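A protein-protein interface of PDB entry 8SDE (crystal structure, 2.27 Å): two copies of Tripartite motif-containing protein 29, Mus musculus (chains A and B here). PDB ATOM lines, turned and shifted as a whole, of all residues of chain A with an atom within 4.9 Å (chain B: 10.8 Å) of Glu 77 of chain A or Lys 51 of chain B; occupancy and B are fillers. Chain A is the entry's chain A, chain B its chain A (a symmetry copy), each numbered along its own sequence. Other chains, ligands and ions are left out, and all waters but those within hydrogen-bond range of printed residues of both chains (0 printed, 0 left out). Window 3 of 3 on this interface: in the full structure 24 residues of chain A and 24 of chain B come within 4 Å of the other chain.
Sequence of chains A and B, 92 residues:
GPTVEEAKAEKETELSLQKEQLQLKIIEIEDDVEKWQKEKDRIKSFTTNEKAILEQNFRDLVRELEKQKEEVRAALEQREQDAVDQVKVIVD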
ATOM      1  N   ARG A  73       9.789 -21.327  19.997  1.00  0.00           N
ATOM      2  CA  ARG A  73      10.732 -21.186  21.091  1.00  0.00           C
ATOM      3  C   ARG A  73      11.838 -22.247  20.997  1.00  0.00           C
ATOM      4  O   ARG A  73      13.036 -21.936  21.134  1.00  0.00           O
ATOM      5  CB  ARG A  73       9.896 -21.199  22.370  1.00  0.00           C
ATOM      6  CG  ARG A  73      10.674 -21.400  23.663  1.00  0.00           C
ATOM      7  CD  ARG A  73       9.798 -21.005  24.852  1.00  0.00           C
ATOM      8  NE  ARG A  73      10.685 -20.981  25.990  1.00  0.00           N
ATOM      9  CZ  ARG A  73      11.004 -19.882  26.657  1.00  0.00           C
ATOM     10  NH1 ARG A  73      10.504 -18.719  26.281  1.00  0.00           N
ATOM     11  NH2 ARG A  73      11.832 -19.949  27.688  1.00  0.00           N
ATOM     12  N   ALA A  74      11.444 -23.504  20.728  1.00  0.00           N
ATOM     13  CA  ALA A  74      12.411 -24.598  20.668  1.00  0.00           C
ATOM     14  C   ALA A  74      13.248 -24.488  19.394  1.00  0.00           C
ATOM     15  O   ALA A  74      14.435 -24.789  19.400  1.00  0.00           O
ATOM     16  CB  ALA A  74      11.698 -25.942  20.782  1.00  0.00           C
ATOM     17  N   ALA A  75      12.659 -24.013  18.299  1.00  0.00           N
ATOM     18  CA  ALA A  75      13.478 -23.610  17.168  1.00  0.00           C
ATOM     19  C   ALA A  75      14.521 -22.559  17.583  1.00  0.00           C
ATOM     20  O   ALA A  75      15.686 -22.716  17.238  1.00  0.00           O
ATOM     21  CB  ALA A  75      12.594 -23.102  16.044  1.00  0.00           C
ATOM     22  N   LEU A  76      14.128 -21.475  18.289  1.00  0.00           N
ATOM     23  CA  LEU A  76      15.099 -20.452  18.693  1.00  0.00           C
ATOM     24  C   LEU A  76      16.241 -21.089  19.488  1.00  0.00           C
ATOM     25  O   LEU A  76      17.385 -20.708  19.303  1.00  0.00           O
ATOM     26  CB  LEU A  76      14.468 -19.349  19.552  1.00  0.00           C
ATOM     27  CG  LEU A  76      13.371 -18.485  18.914  1.00  0.00           C
ATOM     28  CD1 LEU A  76      12.751 -17.568  19.960  1.00  0.00           C
ATOM     29  CD2 LEU A  76      13.918 -17.671  17.752  1.00  0.00           C
ATOM     30  N   GLU A  77      15.920 -22.048  20.369  1.00  0.00           N
ATOM     31  CA  GLU A  77      16.908 -22.689  21.220  1.00  0.00           C
ATOM     32  C   GLU A  77      17.823 -23.635  20.442  1.00  0.00           C
ATOM     33  O   GLU A  77      18.905 -23.958  20.913  1.00  0.00           O
ATOM     34  CB  GLU A  77      16.225 -23.467  22.341  1.00  0.00           C
ATOM     35  CG  GLU A  77      15.902 -22.587  23.526  1.00  0.00           C
ATOM     36  CD  GLU A  77      14.706 -23.048  24.350  1.00  0.00           C
ATOM     37  OE1 GLU A  77      13.934 -23.892  23.846  1.00  0.00           O
ATOM     38  OE2 GLU A  77      14.525 -22.544  25.481  1.00  0.00           O
ATOM     39  N   GLN A  78      17.384 -24.091  19.263  1.00  0.00           N
ATOM     40  CA  GLN A  78      18.193 -25.016  18.492  1.00  0.00           C
ATOM     41  C   GLN A  78      19.113 -24.228  17.572  1.00  0.00           C
ATOM     42  O   GLN A  78      20.221 -24.670  17.305  1.00  0.00           O
ATOM     43  CB  GLN A  78      17.369 -26.052  17.714  1.00  0.00           C
ATOM     44  CG  GLN A  78      17.554 -27.488  18.216  1.00  0.00           C
ATOM     45  CD  GLN A  78      18.985 -27.988  18.177  1.00  0.00           C
ATOM     46  OE1 GLN A  78      19.500 -28.546  19.148  1.00  0.00           O
ATOM     47  NE2 GLN A  78      19.659 -27.781  17.052  1.00  0.00           N
ATOM     48  N   ARG A  79      18.642 -23.089  17.063  1.00  0.00           N
ATOM     49  CA  ARG A  79      19.535 -22.196  16.351  1.00  0.00           C
ATOM     50  C   ARG A  79      20.575 -21.671  17.338  1.00  0.00           C
ATOM     51  O   ARG A  79      21.650 -21.230  16.927  1.00  0.00           O
ATOM     52  CB  ARG A  79      18.769 -21.055  15.673  1.00  0.00           C
ATOM     53  CG  ARG A  79      18.564 -21.259  14.179  1.00  0.00           C
ATOM     54  CD  ARG A  79      17.150 -20.948  13.721  1.00  0.00           C
ATOM     55  NE  ARG A  79      17.120 -20.042  12.577  1.00  0.00           N
ATOM     56  CZ  ARG A  79      17.116 -18.713  12.667  1.00  0.00           C
ATOM     57  NH1 ARG A  79      17.147 -18.123  13.852  1.00  0.00           N
ATOM     58  NH2 ARG A  79      17.092 -17.974  11.570  1.00  0.00           N
ATOM     59  N   GLU A  80      20.243 -21.718  18.639  1.00  0.00           N
ATOM     60  CA  GLU A  80      21.125 -21.111  19.617  1.00  0.00           C
ATOM     61  C   GLU A  80      22.325 -22.022  19.835  1.00  0.00           C
ATOM     62  O   GLU A  80      23.448 -21.582  19.616  1.00  0.00           O
ATOM     63  CB  GLU A  80      20.426 -20.804  20.935  1.00  0.00           C
ATOM     64  CG  GLU A  80      21.317 -20.043  21.900  1.00  0.00           C
ATOM     65  CD  GLU A  80      20.905 -20.185  23.351  1.00  0.00           C
ATOM     66  OE1 GLU A  80      21.306 -19.336  24.154  1.00  0.00           O
ATOM     67  OE2 GLU A  80      20.181 -21.151  23.668  1.00  0.00           O
ATOM     68  N   GLN A  81      22.056 -23.275  20.238  1.00  0.00           N
ATOM     69  CA  GLN A  81      23.076 -24.289  20.469  1.00  0.00           C
ATOM     70  C   GLN A  81      23.869 -24.544  19.192  1.00  0.00           C
ATOM     71  O   GLN A  81      25.087 -24.673  19.241  1.00  0.00           O
ATOM     72  CB  GLN A  81      22.467 -25.560  21.055  1.00  0.00           C
ATOM     73  CG  GLN A  81      22.094 -25.410  22.521  1.00  0.00           C
ATOM     74  CD  GLN A  81      22.078 -26.726  23.260  1.00  0.00           C
ATOM     75  OE1 GLN A  81      22.850 -26.940  24.196  1.00  0.00           O
ATOM     76  NE2 GLN A  81      21.195 -27.624  22.849  1.00  0.00           N
ATOM     77  N   ILE B  43      25.386 -14.584  21.970  1.00  0.00           N
ATOM     78  CA  ILE B  43      24.371 -15.357  21.265  1.00  0.00           C
ATOM     79  C   ILE B  43      23.296 -15.761  22.271  1.00  0.00           C
ATOM     80  O   ILE B  43      22.102 -15.672  21.988  1.00  0.00           O
ATOM     81  CB  ILE B  43      25.025 -16.610  20.637  1.00  0.00           C
ATOM     82  CG1 ILE B  43      26.022 -16.272  19.531  1.00  0.00           C
ATOM     83  CG2 ILE B  43      23.989 -17.626  20.180  1.00  0.00           C
ATOM     84  CD1 ILE B  43      26.865 -17.487  19.091  1.00  0.00           C
ATOM     85  N   LYS B  44      23.737 -16.202  23.452  1.00  0.00           N
ATOM     86  CA  LYS B  44      22.829 -16.507  24.557  1.00  0.00           C
ATOM     87  C   LYS B  44      21.973 -15.307  24.914  1.00  0.00           C
ATOM     88  O   LYS B  44      20.785 -15.398  25.268  1.00  0.00           O
ATOM     89  CB  LYS B  44      23.601 -16.923  25.820  1.00  0.00           C
ATOM     90  CG  LYS B  44      24.012 -18.392  25.846  1.00  0.00           C
ATOM     91  CD  LYS B  44      24.404 -18.943  27.222  1.00  0.00           C
ATOM     92  CE  LYS B  44      24.644 -20.443  27.210  1.00  0.00           C
ATOM     93  NZ  LYS B  44      25.443 -20.906  28.372  1.00  0.00           N
ATOM     94  N   SER B  45      22.622 -14.148  24.909  1.00  0.00           N
ATOM     95  CA  SER B  45      21.937 -12.947  25.317  1.00  0.00           C
ATOM     96  C   SER B  45      20.908 -12.578  24.238  1.00  0.00           C
ATOM     97  O   SER B  45      19.809 -12.123  24.534  1.00  0.00           O
ATOM     98  CB  SER B  45      22.959 -11.878  25.571  1.00  0.00           C
ATOM     99  OG  SER B  45      22.335 -10.703  26.078  1.00  0.00           O
ATOM    100  N   PHE B  46      21.235 -12.820  22.965  1.00  0.00           N
ATOM    101  CA  PHE B  46      20.313 -12.502  21.876  1.00  0.00           C
ATOM    102  C   PHE B  46      19.094 -13.435  21.930  1.00  0.00           C
ATOM    103  O   PHE B  46      17.946 -13.012  21.851  1.00  0.00           O
ATOM    104  CB  PHE B  46      21.065 -12.653  20.551  1.00  0.00           C
ATOM    105  CG  PHE B  46      20.181 -12.649  19.333  1.00  0.00           C
ATOM    106  CD1 PHE B  46      19.574 -13.818  18.896  1.00  0.00           C
ATOM    107  CD2 PHE B  46      19.934 -11.467  18.654  1.00  0.00           C
ATOM    108  CE1 PHE B  46      18.719 -13.794  17.805  1.00  0.00           C
ATOM    109  CE2 PHE B  46      19.073 -11.442  17.569  1.00  0.00           C
ATOM    110  CZ  PHE B  46      18.489 -12.607  17.134  1.00  0.00           C
ATOM    111  N   THR B  47      19.327 -14.707  22.223  1.00  0.00           N
ATOM    112  CA  THR B  47      18.230 -15.654  22.225  1.00  0.00           C
ATOM    113  C   THR B  47      17.249 -15.337  23.330  1.00  0.00           C
ATOM    114  O   THR B  47      16.044 -15.498  23.159  1.00  0.00           O
ATOM    115  CB  THR B  47      18.702 -17.073  22.481  1.00  0.00           C
ATOM    116  OG1 THR B  47      19.720 -17.198  21.495  1.00  0.00           O
ATOM    117  CG2 THR B  47      17.605 -18.084  22.211  1.00  0.00           C
ATOM    118  N   THR B  48      17.789 -14.861  24.443  1.00  0.00           N
ATOM    119  CA  THR B  48      17.006 -14.612  25.638  1.00  0.00           C
ATOM    120  C   THR B  48      16.075 -13.446  25.334  1.00  0.00           C
ATOM    121  O   THR B  48      14.888 -13.451  25.667  1.00  0.00           O
ATOM    122  CB  THR B  48      17.975 -14.350  26.808  1.00  0.00           C
ATOM    123  OG1 THR B  48      18.506 -15.617  27.177  1.00  0.00           O
ATOM    124  CG2 THR B  48      17.371 -13.685  28.020  1.00  0.00           C
ATOM    125  N   ASN B  49      16.645 -12.427  24.710  1.00  0.00           N
ATOM    126  CA  ASN B  49      15.900 -11.266  24.243  1.00  0.00           C
ATOM    127  C   ASN B  49      14.785 -11.664  23.280  1.00  0.00           C
ATOM    128  O   ASN B  49      13.685 -11.147  23.413  1.00  0.00           O
ATOM    129  CB  ASN B  49      16.824 -10.431  23.351  1.00  0.00           C
ATOM    130  CG  ASN B  49      16.909  -8.984  23.756  1.00  0.00           C
ATOM    131  OD1 ASN B  49      15.918  -8.255  23.677  1.00  0.00           O
ATOM    132  ND2 ASN B  49      18.098  -8.573  24.178  1.00  0.00           N
ATOM    133  N   GLU B  50      15.101 -12.486  22.241  1.00  0.00           N
ATOM    134  CA  GLU B  50      14.120 -12.832  21.208  1.00  0.00           C
ATOM    135  C   GLU B  50      12.964 -13.645  21.798  1.00  0.00           C
ATOM    136  O   GLU B  50      11.797 -13.443  21.456  1.00  0.00           O
ATOM    137  CB  GLU B  50      14.785 -13.646  20.085  1.00  0.00           C
ATOM    138  CG  GLU B  50      15.867 -12.857  19.347  1.00  0.00           C
ATOM    139  CD  GLU B  50      15.476 -11.419  18.982  1.00  0.00           C
ATOM    140  OE1 GLU B  50      14.700 -11.253  18.017  1.00  0.00           O
ATOM    141  OE2 GLU B  50      15.935 -10.458  19.667  1.00  0.00           O
ATOM    142  N   LYS B  51      13.282 -14.496  22.780  1.00  0.00           N
ATOM    143  CA  LYS B  51      12.254 -15.298  23.429  1.00  0.00           C
ATOM    144  C   LYS B  51      11.348 -14.424  24.264  1.00  0.00           C
ATOM    145  O   LYS B  51      10.134 -14.632  24.258  1.00  0.00           O
ATOM    146  CB  LYS B  51      12.876 -16.313  24.379  1.00  0.00           C
ATOM    147  CG  LYS B  51      13.406 -17.588  23.738  1.00  0.00           C
ATOM    148  CD  LYS B  51      14.068 -18.414  24.845  1.00  0.00           C
ATOM    149  CE  LYS B  51      14.930 -19.568  24.386  1.00  0.00           C
ATOM    150  NZ  LYS B  51      15.608 -20.222  25.542  1.00  0.00           N
ATOM    151  N   ALA B  52      11.930 -13.396  24.912  1.00  0.00           N
ATOM    152  CA  ALA B  52      11.097 -12.458  25.647  1.00  0.00           C
ATOM    153  C   ALA B  52      10.160 -11.721  24.686  1.00  0.00           C
ATOM    154  O   ALA B  52       9.004 -11.473  25.007  1.00  0.00           O
ATOM    155  CB  ALA B  52      12.007 -11.481  26.350  1.00  0.00           C
ATOM    156  N   ILE B  53      10.662 -11.342  23.494  1.00  0.00           N
ATOM    157  CA  ILE B  53       9.813 -10.599  22.572  1.00  0.00           C
ATOM    158  C   ILE B  53       8.737 -11.532  22.019  1.00  0.00           C
ATOM    159  O   ILE B  53       7.598 -11.136  21.854  1.00  0.00           O
ATOM    160  CB  ILE B  53      10.658  -9.967  21.450  1.00  0.00           C
ATOM    161  CG1 ILE B  53      11.502  -8.797  21.966  1.00  0.00           C
ATOM    162  CG2 ILE B  53       9.767  -9.561  20.293  1.00  0.00           C
ATOM    163  CD1 ILE B  53      12.741  -8.524  21.128  1.00  0.00           C
ATOM    164  N   LEU B  54       9.103 -12.784  21.737  1.00  0.00           N
ATOM    165  CA  LEU B  54       8.114 -13.761  21.306  1.00  0.00           C
ATOM    166  C   LEU B  54       6.988 -13.843  22.339  1.00  0.00           C
ATOM    167  O   LEU B  54       5.796 -13.782  22.010  1.00  0.00           O
ATOM    168  CB  LEU B  54       8.814 -15.112  21.146  1.00  0.00           C
ATOM    169  CG  LEU B  54       7.904 -16.290  20.739  1.00  0.00           C
ATOM    170  CD1 LEU B  54       7.531 -16.182  19.257  1.00  0.00           C
ATOM    171  CD2 LEU B  54       8.627 -17.619  20.912  1.00  0.00           C
ATOM    172  N   GLU B  55       7.380 -14.016  23.603  1.00  0.00           N
ATOM    173  CA  GLU B  55       6.412 -14.188  24.676  1.00  0.00           C
ATOM    174  C   GLU B  55       5.504 -12.972  24.762  1.00  0.00           C
ATOM    175  O   GLU B  55       4.299 -13.112  24.915  1.00  0.00           O
ATOM    176  CB  GLU B  55       7.130 -14.316  26.024  1.00  0.00           C
ATOM    177  CG  GLU B  55       6.293 -15.042  27.040  1.00  0.00           C
ATOM    178  CD  GLU B  55       5.854 -16.402  26.517  1.00  0.00           C
ATOM    179  OE1 GLU B  55       6.738 -17.179  26.055  1.00  0.00           O
ATOM    180  OE2 GLU B  55       4.628 -16.668  26.546  1.00  0.00           O
ATOM    181  N   GLN B  56       6.059 -11.763  24.621  1.00  0.00           N
ATOM    182  CA  GLN B  56       5.187 -10.590  24.620  1.00  0.00           C
ATOM    183  C   GLN B  56       4.305 -10.499  23.355  1.00  0.00           C
ATOM    184  O   GLN B  56       3.169 -10.039  23.408  1.00  0.00           O
ATOM    185  CB  GLN B  56       6.001  -9.321  24.889  1.00  0.00           C
ATOM    186  CG  GLN B  56       5.129  -8.066  25.017  1.00  0.00           C
ATOM    187  CD  GLN B  56       4.180  -8.140  26.200  1.00  0.00           C
ATOM    188  OE1 GLN B  56       4.549  -8.574  27.296  1.00  0.00           O
ATOM    189  NE2 GLN B  56       2.927  -7.757  25.983  1.00  0.00           N
ATOM    190  N   ASN B  57       4.787 -10.925  22.188  1.00  0.00           N
ATOM    191  CA  ASN B  57       3.898 -10.951  21.019  1.00  0.00           C
ATOM    192  C   ASN B  57       2.684 -11.861  21.255  1.00  0.00           C
ATOM    193  O   ASN B  57       1.537 -11.532  20.913  1.00  0.00           O
ATOM    194  CB  ASN B  57       4.665 -11.410  19.764  1.00  0.00           C
ATOM    195  CG  ASN B  57       5.593 -10.327  19.242  1.00  0.00           C
ATOM    196  OD1 ASN B  57       5.694  -9.245  19.826  1.00  0.00           O
ATOM    197  ND2 ASN B  57       6.366 -10.641  18.216  1.00  0.00           N
ATOM    198  N   PHE B  58       2.952 -13.018  21.878  1.00  0.00           N
ATOM    199  CA  PHE B  58       1.942 -14.030  22.099  1.00  0.00           C
ATOM    200  C   PHE B  58       0.858 -13.453  22.999  1.00  0.00           C
ATOM    201  O   PHE B  58      -0.336 -13.597  22.728  1.00  0.00           O
ATOM    202  CB  PHE B  58       2.603 -15.333  22.603  1.00  0.00           C
ATOM    203  CG  PHE B  58       1.610 -16.396  23.001  1.00  0.00           C
ATOM    204  CD1 PHE B  58       0.990 -17.188  22.048  1.00  0.00           C
ATOM    205  CD2 PHE B  58       1.212 -16.538  24.329  1.00  0.00           C
ATOM    206  CE1 PHE B  58      -0.002 -18.096  22.415  1.00  0.00           C
ATOM    207  CE2 PHE B  58       0.261 -17.481  24.707  1.00  0.00           C
ATOM    208  CZ  PHE B  58      -0.327 -18.274  23.744  1.00  0.00           C
ATOM    209  N   ARG B  59       1.281 -12.808  24.085  1.00  0.00           N
ATOM    210  CA  ARG B  59       0.351 -12.200  25.016  1.00  0.00           C
ATOM    211  C   ARG B  59      -0.453 -11.089  24.365  1.00  0.00           C
ATOM    212  O   ARG B  59      -1.646 -10.984  24.649  1.00  0.00           O
ATOM    213  CB  ARG B  59       1.010 -11.635  26.279  1.00  0.00           C
ATOM    214  CG  ARG B  59       1.838 -12.644  27.065  1.00  0.00           C
ATOM    215  CD  ARG B  59       2.143 -11.875  28.351  1.00  0.00           C
ATOM    216  NE  ARG B  59       3.285 -12.446  29.037  1.00  0.00           N
ATOM    217  CZ  ARG B  59       3.302 -13.649  29.606  1.00  0.00           C
ATOM    218  NH1 ARG B  59       2.228 -14.419  29.570  1.00  0.00           N
ATOM    219  NH2 ARG B  59       4.399 -14.083  30.204  1.00  0.00           N
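OE2 of Glu 77 of chain A is in salt-bridge range of NZ of Lys 51 of chain B, 2.6 Å away.
The side-chain hydroxyl (OG1) of Thr 48 of chain B sits at hydrogen-bond distance from the backbone carbonyl oxygen (O) of Lys 44 of chain B.
OG1 of Thr 47 of chain B sits at hydrogen-bond distance from O of Ile 43 of chain B.
Among the printed residues, pairs that only touch across the chains: Arg 73 of chain A with Lys 51 of chain B (3.9 Å), Arg 73 of chain A with Leu 54 of chain B (3.99 Å), Leu 76 of chain A with Thr 47 of chain B (3.9 Å), Leu 76 of chain A with Lys 51 of chain B (3.8 Å), Glu 80 of chain A with Ile 43 of chain B (3.99 Å), Glu 80 of chain A with Lys 44 of chain B (3.2 Å) and Glu 80 of chain A with Thr 47 of chain B (3.3 Å).
Of the printed residues of chain B, Arg 73 of chain A touches Lys 51 and Leu 54.
No residue of chain B comes within 4 Å of Ala 75 of chain A.
Leu 76 of chain A touches just these residues of chain B: Thr 47 and Lys 51.
Glu 77 of chain A touches one residue of chain B.
No residue of chain B comes within 4 Å of Gln 78 of chain A.
Printed residues of chain B within 4 Å of Glu 80 of chain A: Ile 43, Lys 44 and Thr 47.
No residue of chain B comes within 4 Å of Gln 81 of chain A.
Printed residues of chain A within 4 Å of Ile 43 of chain B: Glu 80 (3.99 Å).
Of chain A, only Arg 73, Leu 76 and Glu 77 come within 4 Å of Lys 51 of chain B.
Ala 52 of chain B touches none of the printed residues of chain A.
Of the 9 printed residues of chain A, 4 touch a printed residue of chain B.
Hydrophobic or aromatic side chains of chain A that line the printed part of chain B: Leu 76.
Hydrophobic or aromatic side chains of chain B that line the printed part of chain A: Ile 43 and Leu 54.
No position is printed for both chains.
Of the 8 pairs that touch across the chains among the printed residues, none has its exchanged pair printed and touching as well.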
